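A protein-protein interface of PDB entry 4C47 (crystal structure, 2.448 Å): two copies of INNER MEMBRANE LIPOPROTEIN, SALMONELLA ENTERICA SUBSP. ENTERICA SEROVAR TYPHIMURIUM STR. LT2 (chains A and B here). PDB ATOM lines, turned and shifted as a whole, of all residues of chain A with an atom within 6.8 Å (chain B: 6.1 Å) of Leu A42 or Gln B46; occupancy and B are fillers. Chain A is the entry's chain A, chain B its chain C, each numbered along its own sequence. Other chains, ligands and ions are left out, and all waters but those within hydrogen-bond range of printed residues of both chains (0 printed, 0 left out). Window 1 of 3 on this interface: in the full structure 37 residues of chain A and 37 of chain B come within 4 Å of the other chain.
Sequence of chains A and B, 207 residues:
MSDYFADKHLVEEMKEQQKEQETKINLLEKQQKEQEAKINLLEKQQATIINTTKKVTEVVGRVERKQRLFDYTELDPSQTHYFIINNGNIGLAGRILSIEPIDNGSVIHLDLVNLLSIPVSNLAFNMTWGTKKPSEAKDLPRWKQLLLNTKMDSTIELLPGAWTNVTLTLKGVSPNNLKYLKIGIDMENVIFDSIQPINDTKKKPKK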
ATOM      1  N   GLN A  35     -21.093  26.003  -8.583  1.00  0.00           N
ATOM      2  CA  GLN A  35     -19.827  26.130  -9.300  1.00  0.00           C
ATOM      3  C   GLN A  35     -19.288  24.764  -9.703  1.00  0.00           C
ATOM      4  O   GLN A  35     -18.723  24.606 -10.786  1.00  0.00           O
ATOM      5  CB  GLN A  35     -18.782  26.865  -8.457  1.00  0.00           C
ATOM      6  CG  GLN A  35     -19.029  28.357  -8.329  1.00  0.00           C
ATOM      7  CD  GLN A  35     -17.862  29.084  -7.696  1.00  0.00           C
ATOM      8  OE1 GLN A  35     -16.836  28.478  -7.377  1.00  0.00           O
ATOM      9  NE2 GLN A  35     -18.008  30.390  -7.514  1.00  0.00           N
ATOM     10  N   ALA A  37     -21.136  22.138 -10.390  1.00  0.00           N
ATOM     11  CA  ALA A  37     -21.950  21.755 -11.546  1.00  0.00           C
ATOM     12  C   ALA A  37     -21.456  22.414 -12.842  1.00  0.00           C
ATOM     13  O   ALA A  37     -21.243  21.742 -13.871  1.00  0.00           O
ATOM     14  CB  ALA A  37     -23.416  22.083 -11.292  1.00  0.00           C
ATOM     15  N   LYS A  38     -21.259  23.728 -12.775  1.00  0.00           N
ATOM     16  CA  LYS A  38     -20.770  24.480 -13.929  1.00  0.00           C
ATOM     17  C   LYS A  38     -19.425  23.962 -14.438  1.00  0.00           C
ATOM     18  O   LYS A  38     -19.209  23.857 -15.647  1.00  0.00           O
ATOM     19  CB  LYS A  38     -20.661  25.967 -13.598  1.00  0.00           C
ATOM     20  CG  LYS A  38     -21.999  26.650 -13.371  1.00  0.00           C
ATOM     21  CD  LYS A  38     -21.811  28.126 -13.069  1.00  0.00           C
ATOM     22  CE  LYS A  38     -23.146  28.835 -12.912  1.00  0.00           C
ATOM     23  NZ  LYS A  38     -22.997  30.274 -12.563  1.00  0.00           N
ATOM     24  N   ILE A  39     -18.530  23.631 -13.511  1.00  0.00           N
ATOM     25  CA  ILE A  39     -17.216  23.107 -13.871  1.00  0.00           C
ATOM     26  C   ILE A  39     -17.331  21.759 -14.583  1.00  0.00           C
ATOM     27  O   ILE A  39     -16.665  21.529 -15.600  1.00  0.00           O
ATOM     28  CB  ILE A  39     -16.295  23.007 -12.640  1.00  0.00           C
ATOM     29  CG1 ILE A  39     -15.859  24.406 -12.202  1.00  0.00           C
ATOM     30  CG2 ILE A  39     -15.076  22.154 -12.945  1.00  0.00           C
ATOM     31  CD1 ILE A  39     -15.187  24.437 -10.857  1.00  0.00           C
ATOM     32  N   ASN A  40     -18.179  20.880 -14.054  1.00  0.00           N
ATOM     33  CA  ASN A  40     -18.472  19.613 -14.724  1.00  0.00           C
ATOM     34  C   ASN A  40     -18.879  19.828 -16.178  1.00  0.00           C
ATOM     35  O   ASN A  40     -18.258  19.274 -17.115  1.00  0.00           O
ATOM     36  CB  ASN A  40     -19.583  18.866 -13.987  1.00  0.00           C
ATOM     37  CG  ASN A  40     -19.050  17.789 -13.066  1.00  0.00           C
ATOM     38  OD1 ASN A  40     -18.718  18.051 -11.909  1.00  0.00           O
ATOM     39  ND2 ASN A  40     -18.969  16.566 -13.576  1.00  0.00           N
ATOM     40  N   LEU A  41     -19.918  20.646 -16.355  1.00  0.00           N
ATOM     41  CA  LEU A  41     -20.401  20.979 -17.696  1.00  0.00           C
ATOM     42  C   LEU A  41     -19.281  21.488 -18.598  1.00  0.00           C
ATOM     43  O   LEU A  41     -19.119  21.014 -19.726  1.00  0.00           O
ATOM     44  CB  LEU A  41     -21.529  22.011 -17.630  1.00  0.00           C
ATOM     45  CG  LEU A  41     -22.943  21.442 -17.564  1.00  0.00           C
ATOM     46  CD1 LEU A  41     -23.969  22.562 -17.480  1.00  0.00           C
ATOM     47  CD2 LEU A  41     -23.203  20.560 -18.773  1.00  0.00           C
ATOM     48  N   LEU A  42     -18.504  22.439 -18.087  1.00  0.00           N
ATOM     49  CA  LEU A  42     -17.395  23.019 -18.842  1.00  0.00           C
ATOM     50  C   LEU A  42     -16.376  21.974 -19.285  1.00  0.00           C
ATOM     51  O   LEU A  42     -15.864  22.037 -20.400  1.00  0.00           O
ATOM     52  CB  LEU A  42     -16.701  24.113 -18.029  1.00  0.00           C
ATOM     53  CG  LEU A  42     -17.440  25.447 -17.897  1.00  0.00           C
ATOM     54  CD1 LEU A  42     -16.750  26.345 -16.883  1.00  0.00           C
ATOM     55  CD2 LEU A  42     -17.531  26.136 -19.246  1.00  0.00           C
ATOM     56  N   GLU A  43     -16.081  21.013 -18.416  1.00  0.00           N
ATOM     57  CA  GLU A  43     -15.111  19.975 -18.758  1.00  0.00           C
ATOM     58  C   GLU A  43     -15.626  19.064 -19.874  1.00  0.00           C
ATOM     59  O   GLU A  43     -14.912  18.799 -20.864  1.00  0.00           O
ATOM     60  CB  GLU A  43     -14.715  19.166 -17.518  1.00  0.00           C
ATOM     61  CG  GLU A  43     -13.809  19.933 -16.563  1.00  0.00           C
ATOM     62  CD  GLU A  43     -13.597  19.222 -15.240  1.00  0.00           C
ATOM     63  OE1 GLU A  43     -14.372  18.292 -14.930  1.00  0.00           O
ATOM     64  OE2 GLU A  43     -12.651  19.593 -14.511  1.00  0.00           O
ATOM     65  N   LYS A  44     -16.868  18.603 -19.731  1.00  0.00           N
ATOM     66  CA  LYS A  44     -17.458  17.757 -20.774  1.00  0.00           C
ATOM     67  C   LYS A  44     -17.514  18.481 -22.132  1.00  0.00           C
ATOM     68  O   LYS A  44     -17.069  17.951 -23.176  1.00  0.00           O
ATOM     69  CB  LYS A  44     -18.847  17.286 -20.339  1.00  0.00           C
ATOM     70  CG  LYS A  44     -18.836  16.585 -18.986  1.00  0.00           C
ATOM     71  CD  LYS A  44     -20.195  16.018 -18.617  1.00  0.00           C
ATOM     72  CE  LYS A  44     -20.135  15.302 -17.275  1.00  0.00           C
ATOM     73  NZ  LYS A  44     -21.383  14.541 -17.004  1.00  0.00           N
ATOM     74  N   GLN A  45     -18.041  19.702 -22.102  1.00  0.00           N
ATOM     75  CA  GLN A  45     -18.137  20.531 -23.296  1.00  0.00           C
ATOM     76  C   GLN A  45     -16.773  20.800 -23.915  1.00  0.00           C
ATOM     77  O   GLN A  45     -16.649  20.879 -25.135  1.00  0.00           O
ATOM     78  CB  GLN A  45     -18.848  21.848 -22.978  1.00  0.00           C
ATOM     79  CG  GLN A  45     -20.309  21.664 -22.620  1.00  0.00           C
ATOM     80  CD  GLN A  45     -20.949  22.917 -22.055  1.00  0.00           C
ATOM     81  OE1 GLN A  45     -22.138  22.927 -21.740  1.00  0.00           O
ATOM     82  NE2 GLN A  45     -20.162  23.978 -21.923  1.00  0.00           N
ATOM     83  N   GLN A  46     -15.752  20.928 -23.075  1.00  0.00           N
ATOM     84  CA  GLN A  46     -14.406  21.155 -23.581  1.00  0.00           C
ATOM     85  C   GLN A  46     -13.881  19.925 -24.313  1.00  0.00           C
ATOM     86  O   GLN A  46     -13.250  20.051 -25.365  1.00  0.00           O
ATOM     87  CB  GLN A  46     -13.442  21.570 -22.468  1.00  0.00           C
ATOM     88  CG  GLN A  46     -12.132  22.138 -22.995  1.00  0.00           C
ATOM     89  CD  GLN A  46     -11.281  22.762 -21.912  1.00  0.00           C
ATOM     90  OE1 GLN A  46     -10.736  22.065 -21.056  1.00  0.00           O
ATOM     91  NE2 GLN A  46     -11.164  24.086 -21.940  1.00  0.00           N
ATOM     92  N   ALA A  47     -14.134  18.739 -23.760  1.00  0.00           N
ATOM     93  CA  ALA A  47     -13.748  17.505 -24.455  1.00  0.00           C
ATOM     94  C   ALA A  47     -14.381  17.452 -25.845  1.00  0.00           C
ATOM     95  O   ALA A  47     -13.691  17.207 -26.866  1.00  0.00           O
ATOM     96  CB  ALA A  47     -14.146  16.290 -23.646  1.00  0.00           C
ATOM     97  N   ILE A  49     -15.433  19.963 -27.607  1.00  0.00           N
ATOM     98  CA  ILE A  49     -14.830  21.028 -28.406  1.00  0.00           C
ATOM     99  C   ILE A  49     -13.483  20.614 -29.001  1.00  0.00           C
ATOM    100  O   ILE A  49     -13.223  20.857 -30.178  1.00  0.00           O
ATOM    101  CB  ILE A  49     -14.683  22.340 -27.596  1.00  0.00           C
ATOM    102  CG1 ILE A  49     -16.052  22.988 -27.384  1.00  0.00           C
ATOM    103  CG2 ILE A  49     -13.755  23.316 -28.306  1.00  0.00           C
ATOM    104  CD1 ILE A  49     -16.011  24.233 -26.525  1.00  0.00           C
ATOM    105  N   ILE B  39     -15.119  31.486 -14.309  1.00  0.00           N
ATOM    106  CA  ILE B  39     -16.065  30.523 -14.858  1.00  0.00           C
ATOM    107  C   ILE B  39     -16.961  31.157 -15.918  1.00  0.00           C
ATOM    108  O   ILE B  39     -17.116  30.606 -17.014  1.00  0.00           O
ATOM    109  CB  ILE B  39     -16.923  29.876 -13.747  1.00  0.00           C
ATOM    110  CG1 ILE B  39     -16.104  28.830 -12.985  1.00  0.00           C
ATOM    111  CG2 ILE B  39     -18.177  29.241 -14.333  1.00  0.00           C
ATOM    112  CD1 ILE B  39     -16.800  28.274 -11.760  1.00  0.00           C
ATOM    113  N   LEU B  41     -16.367  33.758 -17.712  1.00  0.00           N
ATOM    114  CA  LEU B  41     -15.487  34.015 -18.846  1.00  0.00           C
ATOM    115  C   LEU B  41     -15.299  32.752 -19.695  1.00  0.00           C
ATOM    116  O   LEU B  41     -15.429  32.790 -20.925  1.00  0.00           O
ATOM    117  CB  LEU B  41     -14.137  34.531 -18.347  1.00  0.00           C
ATOM    118  CG  LEU B  41     -13.466  35.676 -19.113  1.00  0.00           C
ATOM    119  CD1 LEU B  41     -12.229  35.171 -19.833  1.00  0.00           C
ATOM    120  CD2 LEU B  41     -14.430  36.342 -20.090  1.00  0.00           C
ATOM    121  N   LEU B  42     -15.011  31.636 -19.027  1.00  0.00           N
ATOM    122  CA  LEU B  42     -14.859  30.349 -19.705  1.00  0.00           C
ATOM    123  C   LEU B  42     -16.103  29.962 -20.508  1.00  0.00           C
ATOM    124  O   LEU B  42     -15.994  29.541 -21.664  1.00  0.00           O
ATOM    125  CB  LEU B  42     -14.534  29.244 -18.700  1.00  0.00           C
ATOM    126  CG  LEU B  42     -13.136  29.263 -18.081  1.00  0.00           C
ATOM    127  CD1 LEU B  42     -13.026  28.224 -16.973  1.00  0.00           C
ATOM    128  CD2 LEU B  42     -12.080  29.024 -19.147  1.00  0.00           C
ATOM    129  N   GLU B  43     -17.277  30.100 -19.894  1.00  0.00           N
ATOM    130  CA  GLU B  43     -18.531  29.775 -20.572  1.00  0.00           C
ATOM    131  C   GLU B  43     -18.703  30.584 -21.851  1.00  0.00           C
ATOM    132  O   GLU B  43     -18.937  30.023 -22.932  1.00  0.00           O
ATOM    133  CB  GLU B  43     -19.728  30.000 -19.645  1.00  0.00           C
ATOM    134  CG  GLU B  43     -19.856  28.980 -18.528  1.00  0.00           C
ATOM    135  CD  GLU B  43     -20.848  29.405 -17.464  1.00  0.00           C
ATOM    136  OE1 GLU B  43     -21.115  30.619 -17.355  1.00  0.00           O
ATOM    137  OE2 GLU B  43     -21.358  28.528 -16.737  1.00  0.00           O
ATOM    138  N   LYS B  44     -18.577  31.902 -21.729  1.00  0.00           N
ATOM    139  CA  LYS B  44     -18.753  32.761 -22.899  1.00  0.00           C
ATOM    140  C   LYS B  44     -17.753  32.447 -24.020  1.00  0.00           C
ATOM    141  O   LYS B  44     -18.141  32.327 -25.197  1.00  0.00           O
ATOM    142  CB  LYS B  44     -18.724  34.237 -22.498  1.00  0.00           C
ATOM    143  CG  LYS B  44     -19.987  34.657 -21.753  1.00  0.00           C
ATOM    144  CD  LYS B  44     -19.793  35.920 -20.927  1.00  0.00           C
ATOM    145  CE  LYS B  44     -21.040  36.227 -20.107  1.00  0.00           C
ATOM    146  NZ  LYS B  44     -20.829  37.359 -19.161  1.00  0.00           N
ATOM    147  N   GLN B  45     -16.483  32.279 -23.654  1.00  0.00           N
ATOM    148  CA  GLN B  45     -15.473  31.884 -24.633  1.00  0.00           C
ATOM    149  C   GLN B  45     -15.850  30.580 -25.339  1.00  0.00           C
ATOM    150  O   GLN B  45     -15.737  30.477 -26.561  1.00  0.00           O
ATOM    151  CB  GLN B  45     -14.096  31.761 -23.980  1.00  0.00           C
ATOM    152  CG  GLN B  45     -13.482  33.092 -23.584  1.00  0.00           C
ATOM    153  CD  GLN B  45     -12.144  32.937 -22.886  1.00  0.00           C
ATOM    154  OE1 GLN B  45     -11.430  33.917 -22.665  1.00  0.00           O
ATOM    155  NE2 GLN B  45     -11.798  31.705 -22.533  1.00  0.00           N
ATOM    156  N   GLN B  46     -16.313  29.597 -24.569  1.00  0.00           N
ATOM    157  CA  GLN B  46     -16.752  28.324 -25.139  1.00  0.00           C
ATOM    158  C   GLN B  46     -17.875  28.496 -26.158  1.00  0.00           C
ATOM    159  O   GLN B  46     -17.816  27.928 -27.253  1.00  0.00           O
ATOM    160  CB  GLN B  46     -17.189  27.347 -24.047  1.00  0.00           C
ATOM    161  CG  GLN B  46     -16.084  26.417 -23.582  1.00  0.00           C
ATOM    162  CD  GLN B  46     -16.601  25.276 -22.727  1.00  0.00           C
ATOM    163  OE1 GLN B  46     -17.810  25.081 -22.598  1.00  0.00           O
ATOM    164  NE2 GLN B  46     -15.684  24.514 -22.138  1.00  0.00           N
ATOM    165  N   ALA B  47     -18.895  29.276 -25.800  1.00  0.00           N
ATOM    166  CA  ALA B  47     -19.991  29.534 -26.732  1.00  0.00           C
ATOM    167  C   ALA B  47     -19.468  30.145 -28.034  1.00  0.00           C
ATOM    168  O   ALA B  47     -19.807  29.680 -29.133  1.00  0.00           O
ATOM    169  CB  ALA B  47     -21.041  30.432 -26.091  1.00  0.00           C
ATOM    170  N   THR B  48     -18.628  31.170 -27.898  1.00  0.00           N
ATOM    171  CA  THR B  48     -17.988  31.794 -29.055  1.00  0.00           C
ATOM    172  C   THR B  48     -17.287  30.766 -29.950  1.00  0.00           C
ATOM    173  O   THR B  48     -17.505  30.733 -31.170  1.00  0.00           O
ATOM    174  CB  THR B  48     -16.978  32.880 -28.626  1.00  0.00           C
ATOM    175  OG1 THR B  48     -17.684  33.971 -28.024  1.00  0.00           O
ATOM    176  CG2 THR B  48     -16.192  33.392 -29.824  1.00  0.00           C
ATOM    177  N   ILE B  49     -16.462  29.919 -29.337  1.00  0.00           N
ATOM    178  CA  ILE B  49     -15.740  28.882 -30.070  1.00  0.00           C
ATOM    179  C   ILE B  49     -16.687  27.954 -30.832  1.00  0.00           C
ATOM    180  O   ILE B  49     -16.489  27.698 -32.021  1.00  0.00           O
ATOM    181  CB  ILE B  49     -14.834  28.050 -29.141  1.00  0.00           C
ATOM    182  CG1 ILE B  49     -13.714  28.921 -28.570  1.00  0.00           C
ATOM    183  CG2 ILE B  49     -14.237  26.864 -29.892  1.00  0.00           C
ATOM    184  CD1 ILE B  49     -12.906  28.238 -27.482  1.00  0.00           C
ATOM    185  N   ILE B  50     -17.717  27.467 -30.146  1.00  0.00           N
ATOM    186  CA  ILE B  50     -18.700  26.568 -30.751  1.00  0.00           C
ATOM    187  C   ILE B  50     -19.374  27.194 -31.975  1.00  0.00           C
ATOM    188  O   ILE B  50     -19.521  26.551 -33.027  1.00  0.00           O
ATOM    189  CB  ILE B  50     -19.764  26.142 -29.717  1.00  0.00           C
ATOM    190  CG1 ILE B  50     -19.120  25.286 -28.622  1.00  0.00           C
ATOM    191  CG2 ILE B  50     -20.899  25.380 -30.385  1.00  0.00           C
ATOM    192  CD1 ILE B  50     -20.063  24.908 -27.503  1.00  0.00           C
ATOM    193  N   ASN B  51     -19.759  28.459 -31.830  1.00  0.00           N
ATOM    194  CA  ASN B  51     -20.412  29.208 -32.901  1.00  0.00           C
ATOM    195  C   ASN B  51     -19.503  29.391 -34.127  1.00  0.00           C
ATOM    196  O   ASN B  51     -19.885  29.081 -35.270  1.00  0.00           O
ATOM    197  CB  ASN B  51     -20.874  30.564 -32.348  1.00  0.00           C
ATOM    198  CG  ASN B  51     -21.774  31.316 -33.303  1.00  0.00           C
ATOM    199  OD1 ASN B  51     -22.971  31.045 -33.389  1.00  0.00           O
ATOM    200  ND2 ASN B  51     -21.204  32.277 -34.018  1.00  0.00           N
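OE1 of Gln B46 is in hydrogen-bond range of NE2 of Gln A45. The backbone carbonyl oxygen (O) of Leu A42 lies within hydrogen-bond range of the side-chain amide nitrogen (NE2) of Gln B46 (3.0 Å).
Glu B43 touches Lys A38 (OE2 to CD, 3.7 Å). CG of Glu B43 touches CD2 of Leu A42, at 3.7 Å. Gln A46 touches Gln B46. Gln B46 touches Ile A49. CG2 of Ile A49 touches CG2 of Ile B49 (3.9 Å). Ile A49 touches Ile B50 (CD1 to CG1, 3.9 Å).
Printed residues of chain B within 4 Å of Leu A42: Glu B43 and Gln B46. Gln B46 touches four residues of chain A. Printed residues of chain B within 4 Å of Lys A38: Glu B43 (3.7 Å). Printed residues of chain A within 4 Å of Ile B49: Ile A49. Of the printed residues of chain B, Ile A49 touches Gln B46 (3.7 Å), Ile B49 (3.9 Å) and Ile B50 (3.9 Å). Ile B39 touches none of the printed residues of chain A. The nearest printed residue of chain A that does not touch Ile B49 is Gln A46 (7.1 Å).
Printed residues of chain A that touch a printed residue of chain B: Lys A38, Leu A42, Gln A45, Gln A46 and Ile A49. Among the printed residues, 8 pairs touch across the chains.
Leu A42 touches Gln B46, but with the chains exchanged Gln A46 does not touch Leu B42 (5.7 Å). Gln B46 touches its own counterpart, Gln A46. Ile A49 touches Gln B46, but with the chains exchanged Gln A46 does not touch Ile B49 (7.1 Å). Ile A49 touches its own counterpart, Ile B49. Positions printed for both chains: 39, 41, 42, 43, 44, 45, 46, 47 and 49. Of the 8 pairs that touch across the chains among the printed residues, 2 have their exchanged pair printed and touching as well.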
